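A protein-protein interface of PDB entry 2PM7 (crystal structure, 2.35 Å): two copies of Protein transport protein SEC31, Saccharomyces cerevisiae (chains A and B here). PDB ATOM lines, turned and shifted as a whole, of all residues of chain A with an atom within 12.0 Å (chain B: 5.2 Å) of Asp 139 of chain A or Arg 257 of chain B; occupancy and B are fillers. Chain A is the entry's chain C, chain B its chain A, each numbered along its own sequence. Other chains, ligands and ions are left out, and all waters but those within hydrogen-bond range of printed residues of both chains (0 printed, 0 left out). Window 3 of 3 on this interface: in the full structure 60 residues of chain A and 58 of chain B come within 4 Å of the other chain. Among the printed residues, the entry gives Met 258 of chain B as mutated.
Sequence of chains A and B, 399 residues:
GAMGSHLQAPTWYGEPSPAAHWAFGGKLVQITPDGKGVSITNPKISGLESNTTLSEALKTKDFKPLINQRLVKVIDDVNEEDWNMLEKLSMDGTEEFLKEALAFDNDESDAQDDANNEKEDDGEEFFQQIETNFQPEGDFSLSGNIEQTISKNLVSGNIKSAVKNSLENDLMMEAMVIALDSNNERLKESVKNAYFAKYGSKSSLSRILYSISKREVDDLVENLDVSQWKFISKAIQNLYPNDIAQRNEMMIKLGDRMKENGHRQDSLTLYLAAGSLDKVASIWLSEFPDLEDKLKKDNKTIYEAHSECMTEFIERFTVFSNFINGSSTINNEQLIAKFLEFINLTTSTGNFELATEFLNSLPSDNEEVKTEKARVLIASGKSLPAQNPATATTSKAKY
OD1 of Asn 223 of chain B sits close to O of Gly 138 of chain A (3.4 Å). O of Glu 137 of chain A lies within hydrogen-bond range of NH1 of Arg 207 of chain B, 2.8 Å away. The guanidinium group (NH2) of Arg 257 of chain B is in salt-bridge range of the side-chain carboxylate (OD1) of Asp 139 of chain A (3.7 Å). The backbone carbonyl oxygen of Asn 223 of chain B sits at hydrogen-bond distance from the backbone NH of Phe 140 of chain A (3.0 Å). O of Gly 138 of chain A is in hydrogen-bond range of NH2 of Arg 207 of chain B (3.1 Å). The backbone carbonyl oxygen of Phe 140 of chain A lies within hydrogen-bond range of the backbone NH of Asp 225 of chain B, at 2.6 Å.
The backbone carbonyl oxygen (O) of Leu 224 of chain B lies within hydrogen-bond range of the guanidinium group (NH1) of Arg 257 of chain B (2.8 Å). NE of Arg 257 of chain B lies within salt-bridge range of OE2 of Glu 222 of chain B (3.9 Å). O of Val 221 of chain B lies within hydrogen-bond range of NH1 of Arg 257 of chain B (3.3 Å). The side-chain amide nitrogen (ND2) of Asn 261 of chain B is in hydrogen-bond range of the backbone carbonyl oxygen (O) of Arg 257 of chain B.
CB of Pro 136 of chain A touches NH2 of Arg 207 of chain B, 3.5 Å away. CA of Asp 139 of chain A touches O of Asn 223 of chain B, at 3.3 Å. Phe 140 of chain A touches Arg 207 of chain B (CD2 to NH1, 2.9 Å). Leu 224 of chain B touches Phe 140 of chain A (C to O, 3.4 Å). CD1 of Leu 224 of chain B touches CA of Ser 141 of chain A, 3.9 Å away. Ser 141 of chain A touches Asp 225 of chain B.
Gln 135 of chain A touches none of the printed residues of chain B. Printed residues of chain B within 4 Å of Pro 136 of chain A: Arg 207. Of chain B, only Asn 223 and Arg 257 come within 4 Å of Asp 139 of chain A. Printed residues of chain B within 4 Å of Phe 140 of chain A: Arg 207 (2.9 Å), Asn 223 (3.0 Å), Leu 224 (3.4 Å) and Asp 225 (2.6 Å). No residue of chain A comes within 4 Å of Val 221 of chain B. Asn 223 of chain B touches three residues of chain A. Of chain A, only Phe 140 and Ser 141 come within 4 Å of Leu 224 of chain B. Of chain A, only Phe 140 and Ser 141 come within 4 Å of Asp 225 of chain B. No residue of chain A comes within 4 Å of Val 226 of chain B. Gly 255 of chain B touches none of the printed residues of chain A. No residue of chain A comes within 4 Å of Met 258 of chain B. No residue of chain A comes within 4 Å of Glu 260 of chain B. No residue of chain A comes within 4 Å of Asn 261 of chain B.
Of the 18 printed residues of chain B, 5 touch a printed residue of chain A. Hydrophobic or aromatic side chains of chain B that line the printed part of chain A: Leu 224. Among the printed residues, 12 pairs touch across the chains.
No position is printed for both chains. Of the 12 pairs that touch across the chains among the printed residues, none has its exchanged pair printed and touching as well.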
ATOM      1  N   PHE A 134      37.639 -22.182  -7.272  1.00  0.00           N
ATOM      2  CA  PHE A 134      36.311 -21.582  -7.307  1.00  0.00           C
ATOM      3  C   PHE A 134      35.879 -21.160  -5.910  1.00  0.00           C
ATOM      4  O   PHE A 134      35.828 -21.976  -4.985  1.00  0.00           O
ATOM      5  CB  PHE A 134      35.274 -22.550  -7.887  1.00  0.00           C
ATOM      6  CG  PHE A 134      33.870 -21.999  -7.893  1.00  0.00           C
ATOM      7  CD1 PHE A 134      33.595 -20.764  -8.482  1.00  0.00           C
ATOM      8  CD2 PHE A 134      32.826 -22.700  -7.293  1.00  0.00           C
ATOM      9  CE1 PHE A 134      32.304 -20.238  -8.470  1.00  0.00           C
ATOM     10  CE2 PHE A 134      31.532 -22.181  -7.277  1.00  0.00           C
ATOM     11  CZ  PHE A 134      31.271 -20.950  -7.864  1.00  0.00           C
ATOM     12  N   GLN A 135      35.565 -19.877  -5.766  1.00  0.00           N
ATOM     13  CA  GLN A 135      35.138 -19.337  -4.486  1.00  0.00           C
ATOM     14  C   GLN A 135      33.785 -18.653  -4.610  1.00  0.00           C
ATOM     15  O   GLN A 135      33.675 -17.582  -5.204  1.00  0.00           O
ATOM     16  CB  GLN A 135      36.171 -18.333  -3.978  1.00  0.00           C
ATOM     17  CG  GLN A 135      37.588 -18.876  -3.936  1.00  0.00           C
ATOM     18  CD  GLN A 135      38.578 -17.865  -3.391  1.00  0.00           C
ATOM     19  OE1 GLN A 135      38.700 -16.755  -3.912  1.00  0.00           O
ATOM     20  NE2 GLN A 135      39.291 -18.247  -2.335  1.00  0.00           N
ATOM     21  N   PRO A 136      32.733 -19.270  -4.054  1.00  0.00           N
ATOM     22  CA  PRO A 136      31.387 -18.693  -4.113  1.00  0.00           C
ATOM     23  C   PRO A 136      31.422 -17.265  -3.580  1.00  0.00           C
ATOM     24  O   PRO A 136      31.929 -17.019  -2.487  1.00  0.00           O
ATOM     25  CB  PRO A 136      30.580 -19.622  -3.215  1.00  0.00           C
ATOM     26  CG  PRO A 136      31.260 -20.938  -3.407  1.00  0.00           C
ATOM     27  CD  PRO A 136      32.719 -20.561  -3.344  1.00  0.00           C
ATOM     28  N   GLU A 137      30.885 -16.327  -4.352  1.00  0.00           N
ATOM     29  CA  GLU A 137      30.884 -14.925  -3.949  1.00  0.00           C
ATOM     30  C   GLU A 137      29.523 -14.251  -4.043  1.00  0.00           C
ATOM     31  O   GLU A 137      28.729 -14.541  -4.939  1.00  0.00           O
ATOM     32  CB  GLU A 137      31.887 -14.140  -4.801  1.00  0.00           C
ATOM     33  CG  GLU A 137      33.272 -13.976  -4.189  1.00  0.00           C
ATOM     34  CD  GLU A 137      33.299 -12.955  -3.064  1.00  0.00           C
ATOM     35  OE1 GLU A 137      32.703 -13.224  -1.998  1.00  0.00           O
ATOM     36  OE2 GLU A 137      33.911 -11.879  -3.255  1.00  0.00           O
ATOM     37  N   GLY A 138      29.277 -13.338  -3.109  1.00  0.00           N
ATOM     38  CA  GLY A 138      28.033 -12.591  -3.080  1.00  0.00           C
ATOM     39  C   GLY A 138      26.744 -13.390  -3.115  1.00  0.00           C
ATOM     40  O   GLY A 138      26.733 -14.616  -2.961  1.00  0.00           O
ATOM     41  N   ASP A 139      25.647 -12.665  -3.322  1.00  0.00           N
ATOM     42  CA  ASP A 139      24.313 -13.245  -3.389  1.00  0.00           C
ATOM     43  C   ASP A 139      23.975 -13.635  -4.822  1.00  0.00           C
ATOM     44  O   ASP A 139      24.564 -13.125  -5.777  1.00  0.00           O
ATOM     45  CB  ASP A 139      23.279 -12.234  -2.893  1.00  0.00           C
ATOM     46  CG  ASP A 139      23.606 -11.688  -1.517  1.00  0.00           C
ATOM     47  OD1 ASP A 139      23.501 -12.446  -0.526  1.00  0.00           O
ATOM     48  OD2 ASP A 139      23.975 -10.498  -1.431  1.00  0.00           O
ATOM     49  N   PHE A 140      23.016 -14.540  -4.965  1.00  0.00           N
ATOM     50  CA  PHE A 140      22.595 -14.991  -6.279  1.00  0.00           C
ATOM     51  C   PHE A 140      21.235 -15.669  -6.172  1.00  0.00           C
ATOM     52  O   PHE A 140      20.749 -15.941  -5.075  1.00  0.00           O
ATOM     53  CB  PHE A 140      23.639 -15.948  -6.877  1.00  0.00           C
ATOM     54  CG  PHE A 140      23.715 -17.283  -6.187  1.00  0.00           C
ATOM     55  CD1 PHE A 140      23.293 -18.437  -6.839  1.00  0.00           C
ATOM     56  CD2 PHE A 140      24.221 -17.391  -4.891  1.00  0.00           C
ATOM     57  CE1 PHE A 140      23.371 -19.681  -6.214  1.00  0.00           C
ATOM     58  CE2 PHE A 140      24.303 -18.634  -4.253  1.00  0.00           C
ATOM     59  CZ  PHE A 140      23.879 -19.780  -4.915  1.00  0.00           C
ATOM     60  N   SER A 141      20.621 -15.941  -7.314  1.00  0.00           N
ATOM     61  CA  SER A 141      19.310 -16.567  -7.322  1.00  0.00           C
ATOM     62  C   SER A 141      19.095 -17.465  -8.520  1.00  0.00           C
ATOM     63  O   SER A 141      19.755 -17.320  -9.549  1.00  0.00           O
ATOM     64  CB  SER A 141      18.233 -15.489  -7.318  1.00  0.00           C
ATOM     65  OG  SER A 141      18.372 -14.660  -8.456  1.00  0.00           O
ATOM     66  N   LEU A 142      18.162 -18.395  -8.379  1.00  0.00           N
ATOM     67  CA  LEU A 142      17.840 -19.306  -9.461  1.00  0.00           C
ATOM     68  C   LEU A 142      16.829 -18.618 -10.355  1.00  0.00           C
ATOM     69  O   LEU A 142      15.786 -18.168  -9.885  1.00  0.00           O
ATOM     70  CB  LEU A 142      17.244 -20.601  -8.913  1.00  0.00           C
ATOM     71  CG  LEU A 142      18.230 -21.489  -8.152  1.00  0.00           C
ATOM     72  CD1 LEU A 142      17.516 -22.734  -7.635  1.00  0.00           C
ATOM     73  CD2 LEU A 142      19.379 -21.872  -9.084  1.00  0.00           C
ATOM     74  N   SER A 143      17.144 -18.513 -11.639  1.00  0.00           N
ATOM     75  CA  SER A 143      16.227 -17.881 -12.577  1.00  0.00           C
ATOM     76  C   SER A 143      15.847 -18.884 -13.653  1.00  0.00           C
ATOM     77  O   SER A 143      16.691 -19.647 -14.139  1.00  0.00           O
ATOM     78  CB  SER A 143      16.869 -16.649 -13.223  1.00  0.00           C
ATOM     79  OG  SER A 143      17.837 -17.016 -14.194  1.00  0.00           O
ATOM     80  N   GLU A 147      16.687 -23.955 -14.325  1.00  0.00           N
ATOM     81  CA  GLU A 147      17.643 -23.892 -13.227  1.00  0.00           C
ATOM     82  C   GLU A 147      16.962 -24.185 -11.882  1.00  0.00           C
ATOM     83  O   GLU A 147      17.625 -24.579 -10.918  1.00  0.00           O
ATOM     84  CB  GLU A 147      18.314 -22.512 -13.156  1.00  0.00           C
ATOM     85  CG  GLU A 147      19.311 -22.206 -14.274  1.00  0.00           C
ATOM     86  CD  GLU A 147      20.401 -21.209 -13.844  1.00  0.00           C
ATOM     87  OE1 GLU A 147      20.070 -20.159 -13.242  1.00  0.00           O
ATOM     88  OE2 GLU A 147      21.596 -21.472 -14.117  1.00  0.00           O
ATOM     89  N   ARG B 207      26.778 -23.047  -9.717  1.00  0.00           N
ATOM     90  CA  ARG B 207      27.173 -22.732  -8.349  1.00  0.00           C
ATOM     91  C   ARG B 207      26.436 -23.608  -7.337  1.00  0.00           C
ATOM     92  O   ARG B 207      26.961 -23.894  -6.266  1.00  0.00           O
ATOM     93  CB  ARG B 207      26.914 -21.251  -8.043  1.00  0.00           C
ATOM     94  CG  ARG B 207      27.280 -20.841  -6.619  1.00  0.00           C
ATOM     95  CD  ARG B 207      27.087 -19.348  -6.385  1.00  0.00           C
ATOM     96  NE  ARG B 207      27.510 -18.945  -5.045  1.00  0.00           N
ATOM     97  CZ  ARG B 207      27.466 -17.697  -4.592  1.00  0.00           C
ATOM     98  NH1 ARG B 207      27.015 -16.724  -5.368  1.00  0.00           N
ATOM     99  NH2 ARG B 207      27.888 -17.414  -3.366  1.00  0.00           N
ATOM    100  N   LEU B 220      24.695 -21.769  -0.005  1.00  0.00           N
ATOM    101  CA  LEU B 220      23.283 -21.611  -0.298  1.00  0.00           C
ATOM    102  C   LEU B 220      22.576 -20.863   0.822  1.00  0.00           C
ATOM    103  O   LEU B 220      22.089 -19.748   0.638  1.00  0.00           O
ATOM    104  CB  LEU B 220      22.646 -22.987  -0.491  1.00  0.00           C
ATOM    105  CG  LEU B 220      22.943 -23.677  -1.827  1.00  0.00           C
ATOM    106  CD1 LEU B 220      24.405 -23.532  -2.198  1.00  0.00           C
ATOM    107  CD2 LEU B 220      22.553 -25.133  -1.730  1.00  0.00           C
ATOM    108  N   VAL B 221      22.537 -21.494   1.987  1.00  0.00           N
ATOM    109  CA  VAL B 221      21.891 -20.934   3.166  1.00  0.00           C
ATOM    110  C   VAL B 221      22.205 -19.462   3.413  1.00  0.00           C
ATOM    111  O   VAL B 221      21.365 -18.723   3.921  1.00  0.00           O
ATOM    112  CB  VAL B 221      22.287 -21.728   4.431  1.00  0.00           C
ATOM    113  CG1 VAL B 221      21.606 -21.129   5.656  1.00  0.00           C
ATOM    114  CG2 VAL B 221      21.908 -23.196   4.265  1.00  0.00           C
ATOM    115  N   GLU B 222      23.406 -19.035   3.045  1.00  0.00           N
ATOM    116  CA  GLU B 222      23.809 -17.657   3.276  1.00  0.00           C
ATOM    117  C   GLU B 222      23.772 -16.710   2.065  1.00  0.00           C
ATOM    118  O   GLU B 222      23.690 -15.489   2.233  1.00  0.00           O
ATOM    119  CB  GLU B 222      25.213 -17.647   3.900  1.00  0.00           C
ATOM    120  CG  GLU B 222      25.752 -16.260   4.243  1.00  0.00           C
ATOM    121  CD  GLU B 222      24.913 -15.535   5.289  1.00  0.00           C
ATOM    122  OE1 GLU B 222      24.894 -15.987   6.457  1.00  0.00           O
ATOM    123  OE2 GLU B 222      24.270 -14.515   4.942  1.00  0.00           O
ATOM    124  N   ASN B 223      23.814 -17.242   0.849  1.00  0.00           N
ATOM    125  CA  ASN B 223      23.818 -16.355  -0.306  1.00  0.00           C
ATOM    126  C   ASN B 223      22.755 -16.611  -1.372  1.00  0.00           C
ATOM    127  O   ASN B 223      22.530 -15.761  -2.238  1.00  0.00           O
ATOM    128  CB  ASN B 223      25.207 -16.364  -0.948  1.00  0.00           C
ATOM    129  CG  ASN B 223      26.303 -16.019   0.042  1.00  0.00           C
ATOM    130  OD1 ASN B 223      26.440 -14.871   0.466  1.00  0.00           O
ATOM    131  ND2 ASN B 223      27.083 -17.022   0.429  1.00  0.00           N
ATOM    132  N   LEU B 224      22.110 -17.772  -1.328  1.00  0.00           N
ATOM    133  CA  LEU B 224      21.079 -18.052  -2.314  1.00  0.00           C
ATOM    134  C   LEU B 224      19.900 -17.152  -1.997  1.00  0.00           C
ATOM    135  O   LEU B 224      19.583 -16.922  -0.827  1.00  0.00           O
ATOM    136  CB  LEU B 224      20.641 -19.513  -2.267  1.00  0.00           C
ATOM    137  CG  LEU B 224      19.548 -19.873  -3.279  1.00  0.00           C
ATOM    138  CD1 LEU B 224      19.959 -19.412  -4.671  1.00  0.00           C
ATOM    139  CD2 LEU B 224      19.311 -21.368  -3.268  1.00  0.00           C
ATOM    140  N   ASP B 225      19.261 -16.635  -3.038  1.00  0.00           N
ATOM    141  CA  ASP B 225      18.126 -15.748  -2.862  1.00  0.00           C
ATOM    142  C   ASP B 225      17.080 -16.330  -1.916  1.00  0.00           C
ATOM    143  O   ASP B 225      16.632 -17.473  -2.069  1.00  0.00           O
ATOM    144  CB  ASP B 225      17.481 -15.443  -4.210  1.00  0.00           C
ATOM    145  CG  ASP B 225      16.553 -14.255  -4.146  1.00  0.00           C
ATOM    146  OD1 ASP B 225      15.535 -14.331  -3.426  1.00  0.00           O
ATOM    147  OD2 ASP B 225      16.849 -13.237  -4.811  1.00  0.00           O
ATOM    148  N   VAL B 226      16.698 -15.521  -0.935  1.00  0.00           N
ATOM    149  CA  VAL B 226      15.710 -15.917   0.055  1.00  0.00           C
ATOM    150  C   VAL B 226      14.451 -16.482  -0.607  1.00  0.00           C
ATOM    151  O   VAL B 226      13.800 -17.372  -0.065  1.00  0.00           O
ATOM    152  CB  VAL B 226      15.328 -14.713   0.934  1.00  0.00           C
ATOM    153  CG1 VAL B 226      14.249 -15.105   1.905  1.00  0.00           C
ATOM    154  CG2 VAL B 226      16.556 -14.209   1.677  1.00  0.00           C
ATOM    155  N   ILE B 232      16.608 -24.150  -0.030  1.00  0.00           N
ATOM    156  CA  ILE B 232      17.719 -24.080   0.908  1.00  0.00           C
ATOM    157  C   ILE B 232      17.382 -24.918   2.139  1.00  0.00           C
ATOM    158  O   ILE B 232      18.258 -25.283   2.918  1.00  0.00           O
ATOM    159  CB  ILE B 232      17.981 -22.627   1.355  1.00  0.00           C
ATOM    160  CG1 ILE B 232      18.365 -21.777   0.143  1.00  0.00           C
ATOM    161  CG2 ILE B 232      19.091 -22.582   2.409  1.00  0.00           C
ATOM    162  CD1 ILE B 232      18.628 -20.312   0.480  1.00  0.00           C
ATOM    163  N   LYS B 253      19.949 -20.810  11.303  1.00  0.00           N
ATOM    164  CA  LYS B 253      20.746 -19.800  10.619  1.00  0.00           C
ATOM    165  C   LYS B 253      19.930 -19.236   9.461  1.00  0.00           C
ATOM    166  O   LYS B 253      19.996 -18.044   9.157  1.00  0.00           O
ATOM    167  CB  LYS B 253      22.043 -20.443  10.107  1.00  0.00           C
ATOM    168  CG  LYS B 253      23.208 -19.490   9.847  1.00  0.00           C
ATOM    169  CD  LYS B 253      24.511 -20.288   9.716  1.00  0.00           C
ATOM    170  CE  LYS B 253      25.709 -19.410   9.384  1.00  0.00           C
ATOM    171  NZ  LYS B 253      25.606 -18.832   8.018  1.00  0.00           N
ATOM    172  N   LEU B 254      19.149 -20.105   8.827  1.00  0.00           N
ATOM    173  CA  LEU B 254      18.316 -19.697   7.708  1.00  0.00           C
ATOM    174  C   LEU B 254      17.121 -18.910   8.224  1.00  0.00           C
ATOM    175  O   LEU B 254      16.804 -17.839   7.709  1.00  0.00           O
ATOM    176  CB  LEU B 254      17.824 -20.917   6.928  1.00  0.00           C
ATOM    177  CG  LEU B 254      16.857 -20.613   5.773  1.00  0.00           C
ATOM    178  CD1 LEU B 254      17.596 -19.889   4.646  1.00  0.00           C
ATOM    179  CD2 LEU B 254      16.241 -21.910   5.267  1.00  0.00           C
ATOM    180  N   GLY B 255      16.462 -19.455   9.242  1.00  0.00           N
ATOM    181  CA  GLY B 255      15.301 -18.800   9.822  1.00  0.00           C
ATOM    182  C   GLY B 255      15.509 -17.323  10.109  1.00  0.00           C
ATOM    183  O   GLY B 255      14.611 -16.508   9.882  1.00  0.00           O
ATOM    184  N   ASP B 256      16.692 -16.974  10.609  1.00  0.00           N
ATOM    185  CA  ASP B 256      17.003 -15.584  10.919  1.00  0.00           C
ATOM    186  C   ASP B 256      17.052 -14.749   9.647  1.00  0.00           C
ATOM    187  O   ASP B 256      16.515 -13.640   9.592  1.00  0.00           O
ATOM    188  CB  ASP B 256      18.353 -15.473  11.632  1.00  0.00           C
ATOM    189  CG  ASP B 256      18.416 -16.296  12.899  1.00  0.00           C
ATOM    190  OD1 ASP B 256      17.415 -16.322  13.648  1.00  0.00           O
ATOM    191  OD2 ASP B 256      19.477 -16.906  13.152  1.00  0.00           O
ATOM    192  N   ARG B 257      17.706 -15.290   8.626  1.00  0.00           N
ATOM    193  CA  ARG B 257      17.846 -14.598   7.357  1.00  0.00           C
ATOM    194  C   ARG B 257      16.471 -14.278   6.788  1.00  0.00           C
ATOM    195  O   ARG B 257      16.281 -13.246   6.158  1.00  0.00           O
ATOM    196  CB  ARG B 257      18.651 -15.460   6.384  1.00  0.00           C
ATOM    197  CG  ARG B 257      19.260 -14.685   5.238  1.00  0.00           C
ATOM    198  CD  ARG B 257      20.325 -15.489   4.517  1.00  0.00           C
ATOM    199  NE  ARG B 257      20.722 -14.813   3.290  1.00  0.00           N
ATOM    200  CZ  ARG B 257      20.525 -15.296   2.068  1.00  0.00           C
ATOM    201  NH1 ARG B 257      19.942 -16.476   1.903  1.00  0.00           N
ATOM    202  NH2 ARG B 257      20.881 -14.583   1.009  1.00  0.00           N
ATOM    203  N   MET B 258      15.514 -15.168   7.023  1.00  0.00           N
ATOM    204  CA  MET B 258      14.150 -14.971   6.549  1.00  0.00           C
ATOM    205  C   MET B 258      13.529 -13.784   7.275  1.00  0.00           C
ATOM    206  O   MET B 258      13.146 -12.787   6.662  1.00  0.00           O
ATOM    207  CB  MET B 258      13.301 -16.213   6.827  1.00  0.00           C
ATOM    208  CG  MET B 258      13.728 -17.452   6.072  1.00  0.00           C
ATOM    209  SD  MET B 258      13.643 -17.175   4.172  1.00  0.00           S
ATOM    210  CE  MET B 258      11.758 -17.510   3.901  1.00  0.00           C
ATOM    211  N   LYS B 259      13.430 -13.918   8.593  1.00  0.00           N
ATOM    212  CA  LYS B 259      12.856 -12.892   9.453  1.00  0.00           C
ATOM    213  C   LYS B 259      13.437 -11.509   9.179  1.00  0.00           C
ATOM    214  O   LYS B 259      12.705 -10.522   9.104  1.00  0.00           O
ATOM    215  CB  LYS B 259      13.090 -13.268  10.921  1.00  0.00           C
ATOM    216  CG  LYS B 259      12.584 -12.251  11.932  1.00  0.00           C
ATOM    217  CD  LYS B 259      11.082 -12.013  11.792  1.00  0.00           C
ATOM    218  CE  LYS B 259      10.559 -11.105  12.901  1.00  0.00           C
ATOM    219  NZ  LYS B 259      11.306  -9.813  12.990  1.00  0.00           N
ATOM    220  N   GLU B 260      14.755 -11.449   9.026  1.00  0.00           N
ATOM    221  CA  GLU B 260      15.441 -10.186   8.784  1.00  0.00           C
ATOM    222  C   GLU B 260      15.369  -9.732   7.323  1.00  0.00           C
ATOM    223  O   GLU B 260      16.145  -8.886   6.890  1.00  0.00           O
ATOM    224  CB  GLU B 260      16.894 -10.317   9.232  1.00  0.00           C
ATOM    225  CG  GLU B 260      17.628  -9.000   9.365  1.00  0.00           C
ATOM    226  CD  GLU B 260      18.890  -9.132  10.195  1.00  0.00           C
ATOM    227  OE1 GLU B 260      19.729  -9.994   9.858  1.00  0.00           O
ATOM    228  OE2 GLU B 260      19.040  -8.376  11.182  1.00  0.00           O
ATOM    229  N   ASN B 261      14.431 -10.303   6.574  1.00  0.00           N
ATOM    230  CA  ASN B 261      14.234  -9.958   5.171  1.00  0.00           C
ATOM    231  C   ASN B 261      12.756 -10.018   4.814  1.00  0.00           C
ATOM    232  O   ASN B 261      12.386 -10.412   3.705  1.00  0.00           O
ATOM    233  CB  ASN B 261      15.024 -10.899   4.253  1.00  0.00           C
ATOM    234  CG  ASN B 261      16.518 -10.615   4.270  1.00  0.00           C
ATOM    235  OD1 ASN B 261      16.954  -9.489   4.021  1.00  0.00           O
ATOM    236  ND2 ASN B 261      17.311 -11.638   4.561  1.00  0.00           N
